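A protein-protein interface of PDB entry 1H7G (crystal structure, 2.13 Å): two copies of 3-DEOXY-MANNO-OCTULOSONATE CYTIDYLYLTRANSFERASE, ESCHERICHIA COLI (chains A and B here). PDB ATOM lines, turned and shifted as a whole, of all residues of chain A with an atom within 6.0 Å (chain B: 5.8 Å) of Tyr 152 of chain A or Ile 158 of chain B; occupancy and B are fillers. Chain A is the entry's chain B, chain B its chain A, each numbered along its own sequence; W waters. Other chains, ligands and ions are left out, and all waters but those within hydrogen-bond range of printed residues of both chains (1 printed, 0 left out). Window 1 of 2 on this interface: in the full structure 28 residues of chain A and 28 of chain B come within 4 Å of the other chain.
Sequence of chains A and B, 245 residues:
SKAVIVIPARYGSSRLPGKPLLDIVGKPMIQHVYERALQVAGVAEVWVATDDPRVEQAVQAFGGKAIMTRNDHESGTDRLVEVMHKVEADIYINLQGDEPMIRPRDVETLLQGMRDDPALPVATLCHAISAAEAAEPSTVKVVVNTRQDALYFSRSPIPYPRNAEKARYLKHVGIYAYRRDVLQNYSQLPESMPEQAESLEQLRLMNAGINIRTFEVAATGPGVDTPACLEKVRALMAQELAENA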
ATOM      1  N   LYS A 141      32.869  24.737  29.979  1.00  0.00           N
ATOM      2  CA  LYS A 141      31.574  24.909  30.632  1.00  0.00           C
ATOM      3  C   LYS A 141      30.968  23.557  31.024  1.00  0.00           C
ATOM      4  O   LYS A 141      31.201  22.530  30.381  1.00  0.00           O
ATOM      5  CB  LYS A 141      30.595  25.634  29.703  1.00  0.00           C
ATOM      6  CG  LYS A 141      30.736  27.161  29.614  1.00  0.00           C
ATOM      7  CD  LYS A 141      31.967  27.596  28.849  1.00  0.00           C
ATOM      8  CE  LYS A 141      31.931  27.184  27.396  1.00  0.00           C
ATOM      9  NZ  LYS A 141      33.140  27.691  26.683  1.00  0.00           N
ATOM     10  N   VAL A 142      30.193  23.568  32.098  1.00  0.00           N
ATOM     11  CA  VAL A 142      29.529  22.372  32.577  1.00  0.00           C
ATOM     12  C   VAL A 142      28.097  22.737  32.942  1.00  0.00           C
ATOM     13  O   VAL A 142      27.827  23.860  33.392  1.00  0.00           O
ATOM     14  CB  VAL A 142      30.261  21.759  33.820  1.00  0.00           C
ATOM     15  CG1 VAL A 142      30.310  22.761  34.975  1.00  0.00           C
ATOM     16  CG2 VAL A 142      29.590  20.454  34.261  1.00  0.00           C
ATOM     17  N   VAL A 143      27.172  21.824  32.640  1.00  0.00           N
ATOM     18  CA  VAL A 143      25.755  22.004  32.975  1.00  0.00           C
ATOM     19  C   VAL A 143      25.395  20.812  33.852  1.00  0.00           C
ATOM     20  O   VAL A 143      25.739  19.679  33.535  1.00  0.00           O
ATOM     21  CB  VAL A 143      24.840  22.067  31.710  1.00  0.00           C
ATOM     22  CG1 VAL A 143      23.377  22.218  32.116  1.00  0.00           C
ATOM     23  CG2 VAL A 143      25.233  23.249  30.841  1.00  0.00           C
ATOM     24  N   VAL A 144      24.756  21.090  34.982  1.00  0.00           N
ATOM     25  CA  VAL A 144      24.387  20.058  35.950  1.00  0.00           C
ATOM     26  C   VAL A 144      22.877  19.947  36.176  1.00  0.00           C
ATOM     27  O   VAL A 144      22.101  20.789  35.715  1.00  0.00           O
ATOM     28  CB  VAL A 144      25.029  20.349  37.326  1.00  0.00           C
ATOM     29  CG1 VAL A 144      26.515  20.575  37.173  1.00  0.00           C
ATOM     30  CG2 VAL A 144      24.383  21.573  37.961  1.00  0.00           C
ATOM     31  N   ALA A 150      26.906  16.196  36.613  1.00  0.00           N
ATOM     32  CA  ALA A 150      27.193  16.802  35.316  1.00  0.00           C
ATOM     33  C   ALA A 150      26.431  16.115  34.200  1.00  0.00           C
ATOM     34  O   ALA A 150      26.371  14.886  34.138  1.00  0.00           O
ATOM     35  CB  ALA A 150      28.684  16.747  35.026  1.00  0.00           C
ATOM     36  N   LEU A 151      25.813  16.919  33.342  1.00  0.00           N
ATOM     37  CA  LEU A 151      25.086  16.402  32.193  1.00  0.00           C
ATOM     38  C   LEU A 151      26.042  16.330  30.990  1.00  0.00           C
ATOM     39  O   LEU A 151      26.014  15.354  30.235  1.00  0.00           O
ATOM     40  CB  LEU A 151      23.880  17.292  31.862  1.00  0.00           C
ATOM     41  CG  LEU A 151      22.732  17.383  32.875  1.00  0.00           C
ATOM     42  CD1 LEU A 151      21.667  18.330  32.349  1.00  0.00           C
ATOM     43  CD2 LEU A 151      22.146  16.009  33.128  1.00  0.00           C
ATOM     44  N   TYR A 152      26.910  17.338  30.857  1.00  0.00           N
ATOM     45  CA  TYR A 152      27.883  17.418  29.764  1.00  0.00           C
ATOM     46  C   TYR A 152      28.905  18.538  30.026  1.00  0.00           C
ATOM     47  O   TYR A 152      28.635  19.486  30.783  1.00  0.00           O
ATOM     48  CB  TYR A 152      27.144  17.673  28.430  1.00  0.00           C
ATOM     49  CG  TYR A 152      27.995  17.574  27.167  1.00  0.00           C
ATOM     50  CD1 TYR A 152      28.669  16.389  26.840  1.00  0.00           C
ATOM     51  CD2 TYR A 152      28.151  18.679  26.314  1.00  0.00           C
ATOM     52  CE1 TYR A 152      29.477  16.307  25.701  1.00  0.00           C
ATOM     53  CE2 TYR A 152      28.951  18.605  25.176  1.00  0.00           C
ATOM     54  CZ  TYR A 152      29.617  17.420  24.879  1.00  0.00           C
ATOM     55  OH  TYR A 152      30.437  17.365  23.768  1.00  0.00           O
ATOM     56  N   PHE A 153      30.088  18.384  29.428  1.00  0.00           N
ATOM     57  CA  PHE A 153      31.196  19.345  29.521  1.00  0.00           C
ATOM     58  C   PHE A 153      31.491  19.798  28.089  1.00  0.00           C
ATOM     59  O   PHE A 153      31.653  18.957  27.196  1.00  0.00           O
ATOM     60  CB  PHE A 153      32.454  18.666  30.082  1.00  0.00           C
ATOM     61  CG  PHE A 153      32.370  18.324  31.539  1.00  0.00           C
ATOM     62  CD1 PHE A 153      31.857  17.096  31.952  1.00  0.00           C
ATOM     63  CD2 PHE A 153      32.842  19.211  32.501  1.00  0.00           C
ATOM     64  CE1 PHE A 153      31.820  16.750  33.304  1.00  0.00           C
ATOM     65  CE2 PHE A 153      32.809  18.873  33.856  1.00  0.00           C
ATOM     66  CZ  PHE A 153      32.295  17.634  34.254  1.00  0.00           C
ATOM     67  N   SER A 154      31.576  21.109  27.862  1.00  0.00           N
ATOM     68  CA  SER A 154      31.834  21.598  26.513  1.00  0.00           C
ATOM     69  C   SER A 154      32.573  22.923  26.414  1.00  0.00           C
ATOM     70  O   SER A 154      32.621  23.700  27.364  1.00  0.00           O
ATOM     71  CB  SER A 154      30.509  21.721  25.743  1.00  0.00           C
ATOM     72  OG  SER A 154      30.735  21.951  24.362  1.00  0.00           O
ATOM     73  N   SER A 156      31.664  24.811  23.948  1.00  0.00           N
ATOM     74  CA  SER A 156      30.556  25.605  23.405  1.00  0.00           C
ATOM     75  C   SER A 156      29.789  26.202  24.580  1.00  0.00           C
ATOM     76  O   SER A 156      29.726  25.605  25.642  1.00  0.00           O
ATOM     77  CB  SER A 156      29.582  24.728  22.608  1.00  0.00           C
ATOM     78  OG  SER A 156      30.045  24.451  21.302  1.00  0.00           O
ATOM     79  N   ILE A 158      27.158  26.499  26.904  1.00  0.00           N
ATOM     80  CA  ILE A 158      25.977  25.730  27.284  1.00  0.00           C
ATOM     81  C   ILE A 158      25.639  26.168  28.707  1.00  0.00           C
ATOM     82  O   ILE A 158      26.533  26.293  29.552  1.00  0.00           O
ATOM     83  CB  ILE A 158      26.211  24.193  27.227  1.00  0.00           C
ATOM     84  CG1 ILE A 158      27.409  23.797  28.089  1.00  0.00           C
ATOM     85  CG2 ILE A 158      26.396  23.743  25.782  1.00  0.00           C
ATOM     86  CD1 ILE A 158      27.729  22.337  28.031  1.00  0.00           C
ATOM     87  N   PRO A 194      32.972  12.456  21.328  1.00  0.00           N
ATOM     88  CA  PRO A 194      32.878  13.800  21.922  1.00  0.00           C
ATOM     89  C   PRO A 194      34.200  14.222  22.574  1.00  0.00           C
ATOM     90  O   PRO A 194      34.584  15.388  22.503  1.00  0.00           O
ATOM     91  CB  PRO A 194      31.753  13.642  22.959  1.00  0.00           C
ATOM     92  CG  PRO A 194      30.861  12.619  22.326  1.00  0.00           C
ATOM     93  CD  PRO A 194      31.870  11.601  21.823  1.00  0.00           C
ATOM     94  N   GLU A 198      36.057  17.605  21.160  1.00  0.00           N
ATOM     95  CA  GLU A 198      36.185  18.694  22.128  1.00  0.00           C
ATOM     96  C   GLU A 198      37.586  18.825  22.723  1.00  0.00           C
ATOM     97  O   GLU A 198      37.998  19.914  23.116  1.00  0.00           O
ATOM     98  CB  GLU A 198      35.189  18.478  23.276  1.00  0.00           C
ATOM     99  CG  GLU A 198      33.725  18.523  22.863  1.00  0.00           C
ATOM    100  CD  GLU A 198      32.992  19.729  23.421  1.00  0.00           C
ATOM    101  OE1 GLU A 198      33.663  20.660  23.922  1.00  0.00           O
ATOM    102  OE2 GLU A 198      31.744  19.741  23.367  1.00  0.00           O
ATOM    103  N   LEU A 203      35.369  13.494  29.299  1.00  0.00           N
ATOM    104  CA  LEU A 203      34.254  12.960  28.505  1.00  0.00           C
ATOM    105  C   LEU A 203      34.396  11.456  28.241  1.00  0.00           C
ATOM    106  O   LEU A 203      33.439  10.805  27.831  1.00  0.00           O
ATOM    107  CB  LEU A 203      34.099  13.723  27.178  1.00  0.00           C
ATOM    108  CG  LEU A 203      33.713  15.201  27.304  1.00  0.00           C
ATOM    109  CD1 LEU A 203      33.665  15.871  25.947  1.00  0.00           C
ATOM    110  CD2 LEU A 203      32.376  15.323  28.003  1.00  0.00           C
ATOM    111  N   MET A 206      32.174  10.040  30.976  1.00  0.00           N
ATOM    112  CA  MET A 206      30.745  10.194  30.716  1.00  0.00           C
ATOM    113  C   MET A 206      30.258   9.252  29.630  1.00  0.00           C
ATOM    114  O   MET A 206      29.134   8.775  29.687  1.00  0.00           O
ATOM    115  CB  MET A 206      30.434  11.628  30.317  1.00  0.00           C
ATOM    116  CG  MET A 206      30.901  12.649  31.333  1.00  0.00           C
ATOM    117  SD  MET A 206      29.968  14.162  31.143  1.00  0.00           S
ATOM    118  CE  MET A 206      28.559  13.748  32.080  1.00  0.00           C
ATOM    119  N   LYS B 141      20.690  19.737  18.779  1.00  0.00           N
ATOM    120  CA  LYS B 141      21.722  18.710  18.762  1.00  0.00           C
ATOM    121  C   LYS B 141      21.659  17.863  20.030  1.00  0.00           C
ATOM    122  O   LYS B 141      21.160  18.307  21.071  1.00  0.00           O
ATOM    123  CB  LYS B 141      23.118  19.332  18.624  1.00  0.00           C
ATOM    124  CG  LYS B 141      23.527  19.668  17.195  1.00  0.00           C
ATOM    125  CD  LYS B 141      22.743  20.832  16.632  1.00  0.00           C
ATOM    126  CE  LYS B 141      22.930  22.077  17.489  1.00  0.00           C
ATOM    127  NZ  LYS B 141      22.309  23.294  16.900  1.00  0.00           N
ATOM    128  N   VAL B 142      22.143  16.632  19.916  1.00  0.00           N
ATOM    129  CA  VAL B 142      22.189  15.712  21.032  1.00  0.00           C
ATOM    130  C   VAL B 142      23.506  14.939  20.982  1.00  0.00           C
ATOM    131  O   VAL B 142      24.023  14.620  19.906  1.00  0.00           O
ATOM    132  CB  VAL B 142      20.989  14.709  21.024  1.00  0.00           C
ATOM    133  CG1 VAL B 142      20.999  13.870  19.755  1.00  0.00           C
ATOM    134  CG2 VAL B 142      21.027  13.795  22.265  1.00  0.00           C
ATOM    135  N   VAL B 143      24.073  14.713  22.163  1.00  0.00           N
ATOM    136  CA  VAL B 143      25.292  13.939  22.319  1.00  0.00           C
ATOM    137  C   VAL B 143      24.888  12.752  23.204  1.00  0.00           C
ATOM    138  O   VAL B 143      24.224  12.943  24.224  1.00  0.00           O
ATOM    139  CB  VAL B 143      26.415  14.773  22.993  1.00  0.00           C
ATOM    140  CG1 VAL B 143      27.643  13.896  23.243  1.00  0.00           C
ATOM    141  CG2 VAL B 143      26.802  15.940  22.086  1.00  0.00           C
ATOM    142  N   LEU B 151      23.232  12.615  26.738  1.00  0.00           N
ATOM    143  CA  LEU B 151      24.038  13.307  27.743  1.00  0.00           C
ATOM    144  C   LEU B 151      23.483  14.723  27.898  1.00  0.00           C
ATOM    145  O   LEU B 151      23.334  15.231  29.012  1.00  0.00           O
ATOM    146  CB  LEU B 151      25.513  13.372  27.317  1.00  0.00           C
ATOM    147  CG  LEU B 151      26.305  12.062  27.290  1.00  0.00           C
ATOM    148  CD1 LEU B 151      27.761  12.357  26.991  1.00  0.00           C
ATOM    149  CD2 LEU B 151      26.192  11.363  28.635  1.00  0.00           C
ATOM    150  N   TYR B 152      23.164  15.350  26.768  1.00  0.00           N
ATOM    151  CA  TYR B 152      22.619  16.697  26.772  1.00  0.00           C
ATOM    152  C   TYR B 152      22.022  17.026  25.406  1.00  0.00           C
ATOM    153  O   TYR B 152      22.362  16.395  24.406  1.00  0.00           O
ATOM    154  CB  TYR B 152      23.718  17.705  27.133  1.00  0.00           C
ATOM    155  CG  TYR B 152      23.246  19.133  27.368  1.00  0.00           C
ATOM    156  CD1 TYR B 152      22.340  19.434  28.385  1.00  0.00           C
ATOM    157  CD2 TYR B 152      23.697  20.182  26.562  1.00  0.00           C
ATOM    158  CE1 TYR B 152      21.889  20.732  28.592  1.00  0.00           C
ATOM    159  CE2 TYR B 152      23.249  21.494  26.767  1.00  0.00           C
ATOM    160  CZ  TYR B 152      22.343  21.756  27.783  1.00  0.00           C
ATOM    161  OH  TYR B 152      21.875  23.033  27.991  1.00  0.00           O
ATOM    162  N   PHE B 153      21.080  17.969  25.403  1.00  0.00           N
ATOM    163  CA  PHE B 153      20.395  18.471  24.205  1.00  0.00           C
ATOM    164  C   PHE B 153      20.668  19.982  24.173  1.00  0.00           C
ATOM    165  O   PHE B 153      20.504  20.664  25.186  1.00  0.00           O
ATOM    166  CB  PHE B 153      18.875  18.296  24.312  1.00  0.00           C
ATOM    167  CG  PHE B 153      18.406  16.878  24.220  1.00  0.00           C
ATOM    168  CD1 PHE B 153      18.290  16.096  25.364  1.00  0.00           C
ATOM    169  CD2 PHE B 153      18.050  16.334  22.995  1.00  0.00           C
ATOM    170  CE1 PHE B 153      17.823  14.778  25.290  1.00  0.00           C
ATOM    171  CE2 PHE B 153      17.583  15.023  22.900  1.00  0.00           C
ATOM    172  CZ  PHE B 153      17.467  14.241  24.051  1.00  0.00           C
ATOM    173  N   SER B 154      21.009  20.521  23.008  1.00  0.00           N
ATOM    174  CA  SER B 154      21.295  21.947  22.931  1.00  0.00           C
ATOM    175  C   SER B 154      21.164  22.550  21.554  1.00  0.00           C
ATOM    176  O   SER B 154      21.188  21.847  20.541  1.00  0.00           O
ATOM    177  CB  SER B 154      22.715  22.220  23.439  1.00  0.00           C
ATOM    178  OG  SER B 154      23.012  23.610  23.455  1.00  0.00           O
ATOM    179  N   SER B 156      23.293  24.978  20.870  1.00  0.00           N
ATOM    180  CA  SER B 156      24.711  25.261  20.597  1.00  0.00           C
ATOM    181  C   SER B 156      25.263  24.025  19.885  1.00  0.00           C
ATOM    182  O   SER B 156      24.768  22.904  20.079  1.00  0.00           O
ATOM    183  CB  SER B 156      25.533  25.450  21.891  1.00  0.00           C
ATOM    184  OG  SER B 156      25.239  26.655  22.573  1.00  0.00           O
ATOM    185  N   PRO B 157      26.250  24.213  19.001  1.00  0.00           N
ATOM    186  CA  PRO B 157      26.785  23.033  18.328  1.00  0.00           C
ATOM    187  C   PRO B 157      27.620  22.208  19.297  1.00  0.00           C
ATOM    188  O   PRO B 157      28.664  22.665  19.780  1.00  0.00           O
ATOM    189  CB  PRO B 157      27.658  23.637  17.219  1.00  0.00           C
ATOM    190  CG  PRO B 157      26.987  24.910  16.922  1.00  0.00           C
ATOM    191  CD  PRO B 157      26.681  25.439  18.309  1.00  0.00           C
ATOM    192  N   ILE B 158      27.115  21.022  19.633  1.00  0.00           N
ATOM    193  CA  ILE B 158      27.822  20.096  20.512  1.00  0.00           C
ATOM    194  C   ILE B 158      27.960  18.757  19.777  1.00  0.00           C
ATOM    195  O   ILE B 158      27.036  18.312  19.101  1.00  0.00           O
ATOM    196  CB  ILE B 158      27.105  19.885  21.904  1.00  0.00           C
ATOM    197  CG1 ILE B 158      25.649  19.450  21.724  1.00  0.00           C
ATOM    198  CG2 ILE B 158      27.201  21.160  22.761  1.00  0.00           C
ATOM    199  CD1 ILE B 158      24.974  18.981  23.026  1.00  0.00           C
ATOM    200  N   PRO B 159      29.141  18.130  19.849  1.00  0.00           N
ATOM    201  CA  PRO B 159      30.322  18.608  20.574  1.00  0.00           C
ATOM    202  C   PRO B 159      30.981  19.786  19.867  1.00  0.00           C
ATOM    203  O   PRO B 159      30.798  19.982  18.661  1.00  0.00           O
ATOM    204  CB  PRO B 159      31.235  17.391  20.557  1.00  0.00           C
ATOM    205  CG  PRO B 159      30.940  16.784  19.208  1.00  0.00           C
ATOM    206  CD  PRO B 159      29.424  16.844  19.180  1.00  0.00           C
ATOM    207  N   TYR B 160      31.723  20.581  20.630  1.00  0.00           N
ATOM    208  CA  TYR B 160      32.441  21.724  20.072  1.00  0.00           C
ATOM    209  C   TYR B 160      33.475  21.212  19.065  1.00  0.00           C
ATOM    210  O   TYR B 160      34.138  20.208  19.308  1.00  0.00           O
ATOM    211  CB  TYR B 160      33.154  22.488  21.184  1.00  0.00           C
ATOM    212  CG  TYR B 160      33.856  23.720  20.684  1.00  0.00           C
ATOM    213  CD1 TYR B 160      33.130  24.839  20.278  1.00  0.00           C
ATOM    214  CD2 TYR B 160      35.241  23.763  20.596  1.00  0.00           C
ATOM    215  CE1 TYR B 160      33.771  25.971  19.794  1.00  0.00           C
ATOM    216  CE2 TYR B 160      35.895  24.890  20.114  1.00  0.00           C
ATOM    217  CZ  TYR B 160      35.155  25.989  19.713  1.00  0.00           C
ATOM    218  OH  TYR B 160      35.804  27.100  19.222  1.00  0.00           O
ATOM    219  N   ARG B 168      31.122  14.639  14.964  1.00  0.00           N
ATOM    220  CA  ARG B 168      29.991  14.024  14.277  1.00  0.00           C
ATOM    221  C   ARG B 168      28.753  14.542  14.995  1.00  0.00           C
ATOM    222  O   ARG B 168      28.652  14.457  16.220  1.00  0.00           O
ATOM    223  CB  ARG B 168      30.058  12.499  14.342  1.00  0.00           C
ATOM    224  CG  ARG B 168      29.018  11.825  13.467  1.00  0.00           C
ATOM    225  CD  ARG B 168      29.137  10.316  13.515  1.00  0.00           C
ATOM    226  NE  ARG B 168      28.137   9.671  12.664  1.00  0.00           N
ATOM    227  CZ  ARG B 168      26.919   9.313  13.066  1.00  0.00           C
ATOM    228  NH1 ARG B 168      26.526   9.532  14.315  1.00  0.00           N
ATOM    229  NH2 ARG B 168      26.093   8.722  12.214  1.00  0.00           N
ATOM    230  N   TYR B 169      27.825  15.101  14.230  1.00  0.00           N
ATOM    231  CA  TYR B 169      26.622  15.673  14.799  1.00  0.00           C
ATOM    232  C   TYR B 169      25.365  14.835  14.608  1.00  0.00           C
ATOM    233  O   TYR B 169      25.226  14.106  13.621  1.00  0.00           O
ATOM    234  CB  TYR B 169      26.426  17.091  14.253  1.00  0.00           C
ATOM    235  CG  TYR B 169      27.561  18.016  14.628  1.00  0.00           C
ATOM    236  CD1 TYR B 169      27.514  18.758  15.807  1.00  0.00           C
ATOM    237  CD2 TYR B 169      28.712  18.108  13.830  1.00  0.00           C
ATOM    238  CE1 TYR B 169      28.584  19.567  16.192  1.00  0.00           C
ATOM    239  CE2 TYR B 169      29.793  18.922  14.205  1.00  0.00           C
ATOM    240  CZ  TYR B 169      29.718  19.647  15.389  1.00  0.00           C
ATOM    241  OH  TYR B 169      30.762  20.457  15.779  1.00  0.00           O
ATOM    242  N   LEU B 170      24.488  14.910  15.605  1.00  0.00           N
ATOM    243  CA  LEU B 170      23.213  14.199  15.604  1.00  0.00           C
ATOM    244  C   LEU B 170      22.103  15.203  15.825  1.00  0.00           C
ATOM    245  O   LEU B 170      22.152  15.996  16.756  1.00  0.00           O
ATOM    246  CB  LEU B 170      23.152  13.168  16.731  1.00  0.00           C
ATOM    247  CG  LEU B 170      24.006  11.914  16.589  1.00  0.00           C
ATOM    248  CD1 LEU B 170      24.017  11.119  17.899  1.00  0.00           C
ATOM    249  CD2 LEU B 170      23.452  11.089  15.438  1.00  0.00           C
HETATM  250  O   HOH W   1      23.094  13.563  30.862  1.00  0.00           O
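Of the 15 printed residues of chain B, 7 touch a printed residue of chain A.
Hydrophobic or aromatic side chains of chain B that line the printed part of chain A: Val 143, Leu 151, Tyr 152, Ile 158, Pro 159 and Tyr 160.
Among the printed residues, no Asp or Glu carboxylate lies within 4 Å of a Lys or Arg side-chain nitrogen of the other chain.
The side-chain hydroxyl of Tyr 152 of chain A lies within hydrogen-bond range of the side-chain carboxylate of Glu 198 of chain A, at 2.7 Å.
The side-chain hydroxyl of Ser 154 of chain A sits at hydrogen-bond distance from the side-chain carboxylate of Glu 198 of chain A, at 2.6 Å.
The backbone carbonyl oxygen (O) of Tyr 152 of chain A sits at hydrogen-bond distance from the backbone NH (N) of Val 143 of chain A.
O of Pro 159 of chain B sits at hydrogen-bond distance from OH of Tyr 169 of chain B, at 2.9 Å.
The backbone NH (N) of Leu 151 of chain A sits at hydrogen-bond distance from the backbone carbonyl oxygen (O) of Val 143 of chain A, at 2.8 Å.
The backbone NH (N) of Lys 141 of chain A is in hydrogen-bond range of the backbone carbonyl oxygen (O) of Ser 154 of chain A (2.8 Å).
Water W1 bridges the backbone carbonyl oxygen (O) of Leu 151 of chain B (2.5 Å) and the backbone carbonyl oxygen (O) of Leu 151 of chain A (3.5 Å).
Printed residues of chain B within 4 Å of Tyr 152 of chain A: Val 143 (3.9 Å), Tyr 152 (3.7 Å), Ile 158 (3.9 Å) and Pro 159 (3.3 Å).
Ile 158 of chain B touches just these residues of chain A: Tyr 152 and Ser 154.
Of the printed residues of chain B, Ser 154 of chain A touches Ile 158 (3.96 Å).
Of the printed residues of chain B, Leu 151 of chain A touches Leu 151 (2.9 Å).
Printed residues of chain B within 4 Å of Glu 198 of chain A: Pro 159 (3.3 Å) and Tyr 160 (2.9 Å).
The nearest residue of chain B that does not touch Tyr 152 of chain A is Leu 151 of chain B (4.1 Å).
O of Pro 157 of chain B lies within hydrogen-bond range of OG of Ser 156 of chain A, 2.7 Å away.
The backbone carbonyl oxygen (O) of Leu 151 of chain A sits close to the backbone carbonyl oxygen (O) of Leu 151 of chain B, 2.9 Å away.
The backbone NH of Tyr 160 of chain B lies within hydrogen-bond range of the side-chain carboxylate of Glu 198 of chain A, at 2.9 Å.
Among the printed residues, merely in contact across the chains: Ser 156 of chain A with Tyr 160 of chain B (3.3 Å), Tyr 152 of chain A with Pro 159 of chain B (3.3 Å), Glu 198 of chain A with Pro 159 of chain B (3.3 Å), Pro 194 of chain A with Val 143 of chain B (3.6 Å), Tyr 152 of chain A with Tyr 152 of chain B (3.7 Å), Tyr 152 of chain A with Val 143 of chain B (3.9 Å), Tyr 152 of chain A with Ile 158 of chain B (3.9 Å), Ser 154 of chain A with Ile 158 of chain B (3.96 Å) and Ile 158 of chain A with Tyr 152 of chain B (3.99 Å).
Tyr 152 of chain A touches Val 143 of chain B, but with the chains exchanged Val 143 of chain A does not touch Tyr 152 of chain B (4.1 Å).
Tyr 152 of chain B touches its own counterpart, Tyr 152 of chain A.
Tyr 152 of chain A touches Ile 158 of chain B, and with the chains exchanged Ile 158 of chain A touches Tyr 152 of chain B.
Ser 154 of chain A touches Ile 158 of chain B, but with the chains exchanged Ile 158 of chain A does not touch Ser 154 of chain B (4.1 Å).
Positions printed for both chains: 141, 142, 143, 151, 152, 153, 154, 156 and 158.
Of the 12 pairs that touch across the chains among the printed residues, 4 have their exchanged pair printed and touching as well.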
